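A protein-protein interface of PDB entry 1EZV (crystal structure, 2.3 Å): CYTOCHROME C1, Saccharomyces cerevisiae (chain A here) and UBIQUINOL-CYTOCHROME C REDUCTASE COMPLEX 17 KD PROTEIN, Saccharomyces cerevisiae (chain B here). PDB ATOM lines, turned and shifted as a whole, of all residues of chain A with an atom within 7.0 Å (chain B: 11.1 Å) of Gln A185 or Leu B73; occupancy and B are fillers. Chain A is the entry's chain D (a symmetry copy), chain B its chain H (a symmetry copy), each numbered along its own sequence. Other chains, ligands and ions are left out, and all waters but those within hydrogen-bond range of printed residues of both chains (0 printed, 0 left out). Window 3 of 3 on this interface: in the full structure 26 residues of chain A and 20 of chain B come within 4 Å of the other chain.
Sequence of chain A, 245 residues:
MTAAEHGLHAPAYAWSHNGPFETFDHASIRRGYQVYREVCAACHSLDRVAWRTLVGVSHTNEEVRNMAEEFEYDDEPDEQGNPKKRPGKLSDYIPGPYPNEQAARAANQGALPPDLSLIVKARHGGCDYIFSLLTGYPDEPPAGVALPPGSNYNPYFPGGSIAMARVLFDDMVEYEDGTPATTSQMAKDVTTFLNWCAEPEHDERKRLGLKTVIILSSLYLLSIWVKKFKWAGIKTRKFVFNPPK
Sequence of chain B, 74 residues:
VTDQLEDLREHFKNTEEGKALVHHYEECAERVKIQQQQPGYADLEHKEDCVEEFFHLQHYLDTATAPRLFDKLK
The side-chain amino group (NZ) of Lys A188 lies within hydrogen-bond range of the side-chain hydroxyl (OG) of Ser A28, at 3.5 Å. The guanidinium group (NH2) of Arg A31 sits close to the side-chain amide nitrogen (NE2) of Gln A185, 2.9 Å away. NH2 of Arg A31 lies within salt-bridge range of OD1 of Asp A189 (2.7 Å). The side-chain hydroxyl (OG1) of Thr A135 is in hydrogen-bond range of the backbone carbonyl oxygen (O) of Phe A131, 3.0 Å away. The side-chain hydroxyl (OG1) of Thr A182 lies close to the backbone NH (N) of Gln A185. The side-chain carboxylate of Asp A189 lies within hydrogen-bond range of the side-chain amide nitrogen of Gln A185.
Gln A185 touches just these residues of chain B: Leu B73 and Lys B74. Leu B73 touches just these residues of chain A: Ser A184 (3.4 Å), Gln A185 (3.5 Å) and Lys A188 (3.8 Å). No residue of chain B comes within 4 Å of Pro A180. No residue of chain B comes within 4 Å of Ala A181. Thr A182 touches two residues of chain B. No residue of chain B comes within 4 Å of Met A186. No residue of chain B comes within 4 Å of Ala A187. Of chain B, only Phe B70, Leu B73 and Lys B74 come within 4 Å of Lys A188. No residue of chain B comes within 4 Å of Asp A189. Printed residues of chain A within 4 Å of Gln B4: Thr A182 (2.6 Å) and Ser A184 (3.4 Å). Printed residues of chain A within 4 Å of Lys B74: Arg A31, Gln A185 and Lys A188. Lys B72 touches none of the printed residues of chain A. The nearest residue of chain B that does not touch Gln A185 is Gln B4 (4.7 Å). The nearest residue of chain A that does not touch Leu B73 is Thr A182 (4.4 Å).
NH2 of Arg A31 is in salt-bridge range of O of Lys B74 (3.4 Å). OG1 of Thr A182 sits at hydrogen-bond distance from NE2 of Gln B4 (2.6 Å). N of Ser A184 lies within hydrogen-bond range of OD1 of Asp B3, at 3.1 Å. The side-chain hydroxyl (OG) of Ser A184 lies within hydrogen-bond range of the side-chain amide nitrogen (NE2) of Gln B4 (3.4 Å). O of Lys B74 lies within hydrogen-bond range of NE2 of Gln A185 (2.9 Å). O of Lys B74 lies within salt-bridge range of NZ of Lys A188 (3.2 Å).
Phe A131 touches Leu B69. CD2 of Leu B5 touches CB of Thr A135 (3.6 Å). Thr A182 touches Asp B3. Asp B3 touches Thr A183. Ser A184 touches Leu B73 (OG to CD2, 3.4 Å). OE1 of Gln A185 touches CD2 of Leu B73, 3.5 Å away. Phe B70 touches Lys A188. Leu B73 touches Lys A188 (CD1 to CB, 3.8 Å).
Of the 18 printed residues of chain B, 7 touch a printed residue of chain A. Hydrophobic or aromatic side chains of chain B that line the printed part of chain A: Leu B5, Leu B69, Phe B70 and Leu B73. Of the 19 printed residues of chain A, 8 touch a printed residue of chain B. Printed residues of chain A that touch a printed residue of chain B: Arg A31, Phe A131, Thr A135, Thr A182, Thr A183, Ser A184, Gln A185 and Lys A188. Hydrophobic or aromatic side chains of chain A that line the printed part of chain B: Phe A131.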
ATOM      1  N   SER A  28      10.074 -13.701  36.608  1.00  0.00           N
ATOM      2  CA  SER A  28       9.531 -14.359  35.427  1.00  0.00           C
ATOM      3  C   SER A  28       8.996 -15.756  35.755  1.00  0.00           C
ATOM      4  O   SER A  28       7.918 -16.139  35.281  1.00  0.00           O
ATOM      5  CB  SER A  28      10.597 -14.447  34.342  1.00  0.00           C
ATOM      6  OG  SER A  28      10.005 -14.715  33.087  1.00  0.00           O
ATOM      7  N   ARG A  31       5.575 -15.186  37.515  1.00  0.00           N
ATOM      8  CA  ARG A  31       4.571 -14.863  36.506  1.00  0.00           C
ATOM      9  C   ARG A  31       4.189 -16.086  35.676  1.00  0.00           C
ATOM     10  O   ARG A  31       3.002 -16.339  35.444  1.00  0.00           O
ATOM     11  CB  ARG A  31       5.093 -13.763  35.582  1.00  0.00           C
ATOM     12  CG  ARG A  31       4.895 -12.346  36.106  1.00  0.00           C
ATOM     13  CD  ARG A  31       5.406 -11.325  35.105  1.00  0.00           C
ATOM     14  NE  ARG A  31       6.676 -10.742  35.522  1.00  0.00           N
ATOM     15  CZ  ARG A  31       7.762 -10.677  34.763  1.00  0.00           C
ATOM     16  NH1 ARG A  31       8.845 -10.064  35.216  1.00  0.00           N
ATOM     17  NH2 ARG A  31       7.796 -11.283  33.585  1.00  0.00           N
ATOM     18  N   VAL A  35       0.457 -17.898  34.450  1.00  0.00           N
ATOM     19  CA  VAL A  35       0.075 -18.232  33.085  1.00  0.00           C
ATOM     20  C   VAL A  35      -0.220 -19.721  32.976  1.00  0.00           C
ATOM     21  O   VAL A  35      -1.205 -20.116  32.348  1.00  0.00           O
ATOM     22  CB  VAL A  35       1.183 -17.853  32.087  1.00  0.00           C
ATOM     23  CG1 VAL A  35       0.800 -18.295  30.675  1.00  0.00           C
ATOM     24  CG2 VAL A  35       1.434 -16.350  32.130  1.00  0.00           C
ATOM     25  N   PHE A 131       8.892 -21.293  23.229  1.00  0.00           N
ATOM     26  CA  PHE A 131       8.491 -19.920  23.024  1.00  0.00           C
ATOM     27  C   PHE A 131       7.992 -19.722  21.594  1.00  0.00           C
ATOM     28  O   PHE A 131       6.865 -19.268  21.376  1.00  0.00           O
ATOM     29  CB  PHE A 131       9.662 -18.980  23.299  1.00  0.00           C
ATOM     30  CG  PHE A 131       9.304 -17.531  23.170  1.00  0.00           C
ATOM     31  CD1 PHE A 131       8.741 -16.845  24.241  1.00  0.00           C
ATOM     32  CD2 PHE A 131       9.470 -16.865  21.963  1.00  0.00           C
ATOM     33  CE1 PHE A 131       8.348 -15.518  24.108  1.00  0.00           C
ATOM     34  CE2 PHE A 131       9.081 -15.542  21.824  1.00  0.00           C
ATOM     35  CZ  PHE A 131       8.518 -14.866  22.901  1.00  0.00           C
ATOM     36  N   THR A 135       4.154 -18.545  20.075  1.00  0.00           N
ATOM     37  CA  THR A 135       4.011 -17.236  19.462  1.00  0.00           C
ATOM     38  C   THR A 135       4.030 -17.331  17.937  1.00  0.00           C
ATOM     39  O   THR A 135       4.122 -16.317  17.240  1.00  0.00           O
ATOM     40  CB  THR A 135       5.150 -16.306  19.900  1.00  0.00           C
ATOM     41  OG1 THR A 135       6.408 -16.921  19.604  1.00  0.00           O
ATOM     42  CG2 THR A 135       5.066 -16.024  21.389  1.00  0.00           C
ATOM     43  N   LEU A 168      -2.640 -18.275  23.635  1.00  0.00           N
ATOM     44  CA  LEU A 168      -2.187 -17.016  24.207  1.00  0.00           C
ATOM     45  C   LEU A 168      -2.677 -15.846  23.371  1.00  0.00           C
ATOM     46  O   LEU A 168      -2.464 -15.811  22.155  1.00  0.00           O
ATOM     47  CB  LEU A 168      -0.657 -16.977  24.296  1.00  0.00           C
ATOM     48  CG  LEU A 168       0.011 -17.954  25.267  1.00  0.00           C
ATOM     49  CD1 LEU A 168       1.507 -17.678  25.315  1.00  0.00           C
ATOM     50  CD2 LEU A 168      -0.603 -17.815  26.650  1.00  0.00           C
ATOM     51  N   TYR A 175      -1.504  -9.728  35.305  1.00  0.00           N
ATOM     52  CA  TYR A 175      -0.284  -9.970  36.068  1.00  0.00           C
ATOM     53  C   TYR A 175      -0.316  -9.263  37.410  1.00  0.00           C
ATOM     54  O   TYR A 175      -0.537  -8.054  37.489  1.00  0.00           O
ATOM     55  CB  TYR A 175       0.955  -9.531  35.287  1.00  0.00           C
ATOM     56  CG  TYR A 175       1.535 -10.608  34.392  1.00  0.00           C
ATOM     57  CD1 TYR A 175       2.214 -10.274  33.220  1.00  0.00           C
ATOM     58  CD2 TYR A 175       1.356 -11.966  34.690  1.00  0.00           C
ATOM     59  CE1 TYR A 175       2.689 -11.257  32.361  1.00  0.00           C
ATOM     60  CE2 TYR A 175       1.833 -12.957  33.839  1.00  0.00           C
ATOM     61  CZ  TYR A 175       2.493 -12.597  32.674  1.00  0.00           C
ATOM     62  OH  TYR A 175       2.927 -13.566  31.800  1.00  0.00           O
ATOM     63  N   THR A 179       2.836  -5.985  35.213  1.00  0.00           N
ATOM     64  CA  THR A 179       3.454  -6.136  33.893  1.00  0.00           C
ATOM     65  C   THR A 179       2.400  -6.295  32.791  1.00  0.00           C
ATOM     66  O   THR A 179       1.382  -6.969  32.984  1.00  0.00           O
ATOM     67  CB  THR A 179       4.420  -7.354  33.883  1.00  0.00           C
ATOM     68  OG1 THR A 179       5.397  -7.190  34.921  1.00  0.00           O
ATOM     69  CG2 THR A 179       5.135  -7.482  32.540  1.00  0.00           C
ATOM     70  N   PRO A 180       2.588  -5.594  31.657  1.00  0.00           N
ATOM     71  CA  PRO A 180       1.701  -5.754  30.499  1.00  0.00           C
ATOM     72  C   PRO A 180       1.719  -7.190  29.966  1.00  0.00           C
ATOM     73  O   PRO A 180       2.728  -7.660  29.428  1.00  0.00           O
ATOM     74  CB  PRO A 180       2.254  -4.761  29.468  1.00  0.00           C
ATOM     75  CG  PRO A 180       3.134  -3.829  30.243  1.00  0.00           C
ATOM     76  CD  PRO A 180       3.670  -4.629  31.391  1.00  0.00           C
ATOM     77  N   ALA A 181       0.581  -7.859  30.082  1.00  0.00           N
ATOM     78  CA  ALA A 181       0.463  -9.248  29.694  1.00  0.00           C
ATOM     79  C   ALA A 181       0.230  -9.429  28.201  1.00  0.00           C
ATOM     80  O   ALA A 181      -0.770 -10.021  27.790  1.00  0.00           O
ATOM     81  CB  ALA A 181      -0.653  -9.908  30.489  1.00  0.00           C
ATOM     82  N   THR A 182       1.191  -8.992  27.391  1.00  0.00           N
ATOM     83  CA  THR A 182       1.192  -9.316  25.964  1.00  0.00           C
ATOM     84  C   THR A 182       1.491 -10.804  25.737  1.00  0.00           C
ATOM     85  O   THR A 182       1.996 -11.483  26.639  1.00  0.00           O
ATOM     86  CB  THR A 182       2.233  -8.487  25.205  1.00  0.00           C
ATOM     87  OG1 THR A 182       3.534  -8.741  25.749  1.00  0.00           O
ATOM     88  CG2 THR A 182       1.917  -6.999  25.321  1.00  0.00           C
ATOM     89  N   THR A 183       1.178 -11.309  24.542  1.00  0.00           N
ATOM     90  CA  THR A 183       1.291 -12.744  24.282  1.00  0.00           C
ATOM     91  C   THR A 183       2.743 -13.214  24.332  1.00  0.00           C
ATOM     92  O   THR A 183       3.034 -14.281  24.873  1.00  0.00           O
ATOM     93  CB  THR A 183       0.676 -13.159  22.915  1.00  0.00           C
ATOM     94  OG1 THR A 183       1.671 -13.084  21.887  1.00  0.00           O
ATOM     95  CG2 THR A 183      -0.497 -12.266  22.553  1.00  0.00           C
ATOM     96  N   SER A 184       3.652 -12.375  23.841  1.00  0.00           N
ATOM     97  CA  SER A 184       5.068 -12.715  23.820  1.00  0.00           C
ATOM     98  C   SER A 184       5.679 -12.600  25.213  1.00  0.00           C
ATOM     99  O   SER A 184       6.650 -13.287  25.535  1.00  0.00           O
ATOM    100  CB  SER A 184       5.822 -11.814  22.833  1.00  0.00           C
ATOM    101  OG  SER A 184       6.097 -10.544  23.398  1.00  0.00           O
ATOM    102  N   GLN A 185       5.095 -11.740  26.042  1.00  0.00           N
ATOM    103  CA  GLN A 185       5.504 -11.616  27.438  1.00  0.00           C
ATOM    104  C   GLN A 185       5.063 -12.840  28.233  1.00  0.00           C
ATOM    105  O   GLN A 185       5.810 -13.346  29.069  1.00  0.00           O
ATOM    106  CB  GLN A 185       4.900 -10.353  28.053  1.00  0.00           C
ATOM    107  CG  GLN A 185       5.132 -10.210  29.538  1.00  0.00           C
ATOM    108  CD  GLN A 185       6.532  -9.754  29.880  1.00  0.00           C
ATOM    109  OE1 GLN A 185       7.080  -8.845  29.254  1.00  0.00           O
ATOM    110  NE2 GLN A 185       7.095 -10.339  30.924  1.00  0.00           N
ATOM    111  N   MET A 186       3.837 -13.290  27.991  1.00  0.00           N
ATOM    112  CA  MET A 186       3.307 -14.459  28.673  1.00  0.00           C
ATOM    113  C   MET A 186       4.035 -15.722  28.233  1.00  0.00           C
ATOM    114  O   MET A 186       4.362 -16.570  29.055  1.00  0.00           O
ATOM    115  CB  MET A 186       1.813 -14.600  28.401  1.00  0.00           C
ATOM    116  CG  MET A 186       0.967 -13.562  29.118  1.00  0.00           C
ATOM    117  SD  MET A 186      -0.771 -13.861  28.874  1.00  0.00           S
ATOM    118  CE  MET A 186      -0.908 -13.473  27.133  1.00  0.00           C
ATOM    119  N   ALA A 187       4.341 -15.806  26.941  1.00  0.00           N
ATOM    120  CA  ALA A 187       5.118 -16.909  26.404  1.00  0.00           C
ATOM    121  C   ALA A 187       6.497 -16.946  27.054  1.00  0.00           C
ATOM    122  O   ALA A 187       6.908 -17.978  27.577  1.00  0.00           O
ATOM    123  CB  ALA A 187       5.248 -16.765  24.906  1.00  0.00           C
ATOM    124  N   LYS A 188       7.144 -15.785  27.128  1.00  0.00           N
ATOM    125  CA  LYS A 188       8.460 -15.669  27.750  1.00  0.00           C
ATOM    126  C   LYS A 188       8.434 -16.158  29.196  1.00  0.00           C
ATOM    127  O   LYS A 188       9.325 -16.888  29.618  1.00  0.00           O
ATOM    128  CB  LYS A 188       8.949 -14.216  27.692  1.00  0.00           C
ATOM    129  CG  LYS A 188      10.380 -13.987  28.177  1.00  0.00           C
ATOM    130  CD  LYS A 188      10.414 -13.405  29.585  1.00  0.00           C
ATOM    131  CE  LYS A 188      11.692 -12.623  29.844  1.00  0.00           C
ATOM    132  NZ  LYS A 188      11.925 -12.436  31.313  1.00  0.00           N
ATOM    133  N   ASP A 189       7.343 -15.867  29.899  1.00  0.00           N
ATOM    134  CA  ASP A 189       7.226 -16.207  31.311  1.00  0.00           C
ATOM    135  C   ASP A 189       6.953 -17.689  31.582  1.00  0.00           C
ATOM    136  O   ASP A 189       7.596 -18.259  32.459  1.00  0.00           O
ATOM    137  CB  ASP A 189       6.144 -15.347  31.992  1.00  0.00           C
ATOM    138  CG  ASP A 189       6.530 -13.867  32.097  1.00  0.00           C
ATOM    139  OD1 ASP A 189       7.730 -13.526  32.001  1.00  0.00           O
ATOM    140  OD2 ASP A 189       5.617 -13.034  32.279  1.00  0.00           O
ATOM    141  N   VAL A 190       5.952 -18.290  30.925  1.00  0.00           N
ATOM    142  CA  VAL A 190       5.668 -19.712  31.171  1.00  0.00           C
ATOM    143  C   VAL A 190       6.892 -20.528  30.811  1.00  0.00           C
ATOM    144  O   VAL A 190       7.188 -21.535  31.444  1.00  0.00           O
ATOM    145  CB  VAL A 190       4.524 -20.313  30.316  1.00  0.00           C
ATOM    146  CG1 VAL A 190       3.316 -20.551  31.158  1.00  0.00           C
ATOM    147  CG2 VAL A 190       4.241 -19.480  29.114  1.00  0.00           C
ATOM    148  N   VAL B   1      -1.044  -2.919  25.864  1.00  0.00           N
ATOM    149  CA  VAL B   1      -0.320  -2.394  24.667  1.00  0.00           C
ATOM    150  C   VAL B   1      -0.419  -3.404  23.524  1.00  0.00           C
ATOM    151  O   VAL B   1      -1.133  -4.406  23.631  1.00  0.00           O
ATOM    152  CB  VAL B   1       1.183  -2.131  24.973  1.00  0.00           C
ATOM    153  CG1 VAL B   1       1.687  -0.959  24.142  1.00  0.00           C
ATOM    154  CG2 VAL B   1       1.392  -1.855  26.459  1.00  0.00           C
ATOM    155  N   THR B   2       0.240  -3.097  22.408  1.00  0.00           N
ATOM    156  CA  THR B   2       0.337  -4.024  21.284  1.00  0.00           C
ATOM    157  C   THR B   2       1.513  -4.987  21.495  1.00  0.00           C
ATOM    158  O   THR B   2       2.556  -4.600  22.040  1.00  0.00           O
ATOM    159  CB  THR B   2       0.506  -3.252  19.943  1.00  0.00           C
ATOM    160  OG1 THR B   2       0.523  -4.177  18.848  1.00  0.00           O
ATOM    161  CG2 THR B   2       1.800  -2.439  19.944  1.00  0.00           C
ATOM    162  N   ASP B   3       1.316  -6.250  21.114  1.00  0.00           N
ATOM    163  CA  ASP B   3       2.340  -7.283  21.277  1.00  0.00           C
ATOM    164  C   ASP B   3       3.675  -6.899  20.638  1.00  0.00           C
ATOM    165  O   ASP B   3       3.725  -6.512  19.470  1.00  0.00           O
ATOM    166  CB  ASP B   3       1.856  -8.615  20.694  1.00  0.00           C
ATOM    167  CG  ASP B   3       2.899  -9.716  20.812  1.00  0.00           C
ATOM    168  OD1 ASP B   3       3.388  -9.951  21.937  1.00  0.00           O
ATOM    169  OD2 ASP B   3       3.253 -10.321  19.774  1.00  0.00           O
ATOM    170  N   GLN B   4       4.756  -7.107  21.386  1.00  0.00           N
ATOM    171  CA  GLN B   4       6.079  -6.613  21.020  1.00  0.00           C
ATOM    172  C   GLN B   4       6.696  -7.383  19.855  1.00  0.00           C
ATOM    173  O   GLN B   4       7.495  -6.835  19.092  1.00  0.00           O
ATOM    174  CB  GLN B   4       7.011  -6.676  22.231  1.00  0.00           C
ATOM    175  CG  GLN B   4       6.630  -5.746  23.378  1.00  0.00           C
ATOM    176  CD  GLN B   4       5.777  -6.414  24.449  1.00  0.00           C
ATOM    177  OE1 GLN B   4       5.845  -6.049  25.625  1.00  0.00           O
ATOM    178  NE2 GLN B   4       4.951  -7.372  24.047  1.00  0.00           N
ATOM    179  N   LEU B   5       6.340  -8.659  19.738  1.00  0.00           N
ATOM    180  CA  LEU B   5       6.807  -9.496  18.641  1.00  0.00           C
ATOM    181  C   LEU B   5       6.063  -9.150  17.349  1.00  0.00           C
ATOM    182  O   LEU B   5       6.685  -8.955  16.301  1.00  0.00           O
ATOM    183  CB  LEU B   5       6.605 -10.977  18.990  1.00  0.00           C
ATOM    184  CG  LEU B   5       7.118 -12.039  18.013  1.00  0.00           C
ATOM    185  CD1 LEU B   5       8.609 -11.880  17.782  1.00  0.00           C
ATOM    186  CD2 LEU B   5       6.817 -13.410  18.573  1.00  0.00           C
ATOM    187  N   GLU B   6       4.738  -9.050  17.441  1.00  0.00           N
ATOM    188  CA  GLU B   6       3.899  -8.629  16.320  1.00  0.00           C
ATOM    189  C   GLU B   6       4.354  -7.286  15.760  1.00  0.00           C
ATOM    190  O   GLU B   6       4.320  -7.064  14.549  1.00  0.00           O
ATOM    191  CB  GLU B   6       2.441  -8.518  16.764  1.00  0.00           C
ATOM    192  CG  GLU B   6       1.628  -9.777  16.550  1.00  0.00           C
ATOM    193  CD  GLU B   6       0.391  -9.527  15.709  1.00  0.00           C
ATOM    194  OE1 GLU B   6      -0.671  -9.211  16.293  1.00  0.00           O
ATOM    195  OE2 GLU B   6       0.488  -9.626  14.463  1.00  0.00           O
ATOM    196  N   ASP B   7       4.770  -6.399  16.659  1.00  0.00           N
ATOM    197  CA  ASP B   7       5.288  -5.085  16.300  1.00  0.00           C
ATOM    198  C   ASP B   7       6.565  -5.203  15.469  1.00  0.00           C
ATOM    199  O   ASP B   7       6.651  -4.648  14.375  1.00  0.00           O
ATOM    200  CB  ASP B   7       5.566  -4.279  17.572  1.00  0.00           C
ATOM    201  CG  ASP B   7       6.052  -2.869  17.282  1.00  0.00           C
ATOM    202  OD1 ASP B   7       5.209  -1.944  17.274  1.00  0.00           O
ATOM    203  OD2 ASP B   7       7.278  -2.682  17.105  1.00  0.00           O
ATOM    204  N   LEU B   8       7.544  -5.938  15.992  1.00  0.00           N
ATOM    205  CA  LEU B   8       8.837  -6.105  15.330  1.00  0.00           C
ATOM    206  C   LEU B   8       8.740  -6.899  14.026  1.00  0.00           C
ATOM    207  O   LEU B   8       9.522  -6.680  13.097  1.00  0.00           O
ATOM    208  CB  LEU B   8       9.832  -6.778  16.281  1.00  0.00           C
ATOM    209  CG  LEU B   8      10.577  -5.858  17.248  1.00  0.00           C
ATOM    210  CD1 LEU B   8      11.350  -6.686  18.255  1.00  0.00           C
ATOM    211  CD2 LEU B   8      11.519  -4.957  16.471  1.00  0.00           C
ATOM    212  N   THR B  65      14.103 -10.461  14.422  1.00  0.00           N
ATOM    213  CA  THR B  65      13.329 -10.191  15.630  1.00  0.00           C
ATOM    214  C   THR B  65      13.910 -10.833  16.893  1.00  0.00           C
ATOM    215  O   THR B  65      13.848 -10.252  17.977  1.00  0.00           O
ATOM    216  CB  THR B  65      11.863 -10.650  15.471  1.00  0.00           C
ATOM    217  OG1 THR B  65      11.824 -12.052  15.190  1.00  0.00           O
ATOM    218  CG2 THR B  65      11.190  -9.897  14.339  1.00  0.00           C
ATOM    219  N   ALA B  66      14.544 -11.993  16.731  1.00  0.00           N
ATOM    220  CA  ALA B  66      15.033 -12.776  17.862  1.00  0.00           C
ATOM    221  C   ALA B  66      16.080 -12.082  18.736  1.00  0.00           C
ATOM    222  O   ALA B  66      16.047 -12.209  19.963  1.00  0.00           O
ATOM    223  CB  ALA B  66      15.562 -14.124  17.377  1.00  0.00           C
ATOM    224  N   PRO B  67      17.040 -11.364  18.126  1.00  0.00           N
ATOM    225  CA  PRO B  67      18.052 -10.694  18.954  1.00  0.00           C
ATOM    226  C   PRO B  67      17.565  -9.427  19.663  1.00  0.00           C
ATOM    227  O   PRO B  67      18.271  -8.872  20.505  1.00  0.00           O
ATOM    228  CB  PRO B  67      19.179 -10.390  17.963  1.00  0.00           C
ATOM    229  CG  PRO B  67      18.504 -10.334  16.643  1.00  0.00           C
ATOM    230  CD  PRO B  67      17.438 -11.388  16.708  1.00  0.00           C
ATOM    231  N   ARG B  68      16.326  -9.031  19.388  1.00  0.00           N
ATOM    232  CA  ARG B  68      15.834  -7.719  19.793  1.00  0.00           C
ATOM    233  C   ARG B  68      14.625  -7.793  20.713  1.00  0.00           C
ATOM    234  O   ARG B  68      14.432  -6.916  21.555  1.00  0.00           O
ATOM    235  CB  ARG B  68      15.480  -6.886  18.554  1.00  0.00           C
ATOM    236  CG  ARG B  68      16.627  -6.050  18.009  1.00  0.00           C
ATOM    237  CD  ARG B  68      16.183  -5.197  16.826  1.00  0.00           C
ATOM    238  NE  ARG B  68      16.235  -5.940  15.570  1.00  0.00           N
ATOM    239  CZ  ARG B  68      17.231  -5.861  14.691  1.00  0.00           C
ATOM    240  NH1 ARG B  68      17.230  -6.645  13.618  1.00  0.00           N
ATOM    241  NH2 ARG B  68      18.219  -4.990  14.868  1.00  0.00           N
ATOM    242  N   LEU B  69      13.836  -8.856  20.581  1.00  0.00           N
ATOM    243  CA  LEU B  69      12.543  -8.940  21.252  1.00  0.00           C
ATOM    244  C   LEU B  69      12.607  -8.814  22.781  1.00  0.00           C
ATOM    245  O   LEU B  69      11.730  -8.195  23.393  1.00  0.00           O
ATOM    246  CB  LEU B  69      11.837 -10.242  20.870  1.00  0.00           C
ATOM    247  CG  LEU B  69      10.511 -10.506  21.586  1.00  0.00           C
ATOM    248  CD1 LEU B  69       9.544  -9.361  21.312  1.00  0.00           C
ATOM    249  CD2 LEU B  69       9.926 -11.829  21.131  1.00  0.00           C
ATOM    250  N   PHE B  70      13.643  -9.383  23.393  1.00  0.00           N
ATOM    251  CA  PHE B  70      13.692  -9.478  24.849  1.00  0.00           C
ATOM    252  C   PHE B  70      14.175  -8.199  25.547  1.00  0.00           C
ATOM    253  O   PHE B  70      13.871  -7.975  26.722  1.00  0.00           O
ATOM    254  CB  PHE B  70      14.539 -10.689  25.275  1.00  0.00           C
ATOM    255  CG  PHE B  70      13.787 -12.001  25.236  1.00  0.00           C
ATOM    256  CD1 PHE B  70      12.825 -12.243  24.260  1.00  0.00           C
ATOM    257  CD2 PHE B  70      14.025 -12.981  26.187  1.00  0.00           C
ATOM    258  CE1 PHE B  70      12.111 -13.443  24.235  1.00  0.00           C
ATOM    259  CE2 PHE B  70      13.321 -14.182  26.169  1.00  0.00           C
ATOM    260  CZ  PHE B  70      12.359 -14.413  25.191  1.00  0.00           C
ATOM    261  N   ASP B  71      14.848  -7.324  24.805  1.00  0.00           N
ATOM    262  CA  ASP B  71      15.133  -5.980  25.301  1.00  0.00           C
ATOM    263  C   ASP B  71      13.854  -5.154  25.444  1.00  0.00           C
ATOM    264  O   ASP B  71      13.820  -4.171  26.183  1.00  0.00           O
ATOM    265  CB  ASP B  71      16.111  -5.258  24.372  1.00  0.00           C
ATOM    266  CG  ASP B  71      17.546  -5.696  24.586  1.00  0.00           C
ATOM    267  OD1 ASP B  71      18.238  -5.958  23.578  1.00  0.00           O
ATOM    268  OD2 ASP B  71      17.986  -5.776  25.758  1.00  0.00           O
ATOM    269  N   LYS B  72      12.791  -5.587  24.776  1.00  0.00           N
ATOM    270  CA  LYS B  72      11.501  -4.922  24.886  1.00  0.00           C
ATOM    271  C   LYS B  72      10.584  -5.593  25.909  1.00  0.00           C
ATOM    272  O   LYS B  72       9.577  -5.020  26.315  1.00  0.00           O
ATOM    273  CB  LYS B  72      10.815  -4.862  23.516  1.00  0.00           C
ATOM    274  CG  LYS B  72      11.524  -3.961  22.504  1.00  0.00           C
ATOM    275  CD  LYS B  72      11.867  -2.596  23.111  1.00  0.00           C
ATOM    276  CE  LYS B  72      12.505  -1.662  22.089  1.00  0.00           C
ATOM    277  NZ  LYS B  72      11.542  -1.245  21.021  1.00  0.00           N
ATOM    278  N   LEU B  73      10.949  -6.797  26.340  1.00  0.00           N
ATOM    279  CA  LEU B  73      10.178  -7.514  27.348  1.00  0.00           C
ATOM    280  C   LEU B  73      10.742  -7.284  28.745  1.00  0.00           C
ATOM    281  O   LEU B  73      11.861  -6.796  28.903  1.00  0.00           O
ATOM    282  CB  LEU B  73      10.157  -9.014  27.043  1.00  0.00           C
ATOM    283  CG  LEU B  73       9.413  -9.469  25.785  1.00  0.00           C
ATOM    284  CD1 LEU B  73       9.464 -10.985  25.683  1.00  0.00           C
ATOM    285  CD2 LEU B  73       7.972  -8.996  25.832  1.00  0.00           C
ATOM    286  N   LYS B  74       9.928  -7.579  29.753  1.00  0.00           N
ATOM    287  CA  LYS B  74      10.368  -7.507  31.139  1.00  0.00           C
ATOM    288  C   LYS B  74      10.718  -8.909  31.643  1.00  0.00           C
ATOM    289  O   LYS B  74       9.960  -9.860  31.344  1.00  0.00           O
ATOM    290  CB  LYS B  74       9.272  -6.856  32.005  1.00  0.00           C
ATOM    291  CG  LYS B  74       9.353  -7.137  33.515  1.00  0.00           C
ATOM    292  CD  LYS B  74      10.633  -6.592  34.169  1.00  0.00           C
ATOM    293  CE  LYS B  74      10.936  -7.302  35.500  1.00  0.00           C
ATOM    294  NZ  LYS B  74      11.321  -8.745  35.329  1.00  0.00           N
ATOM    295  OXT LYS B  74      11.791  -9.045  32.269  1.00  0.00           O
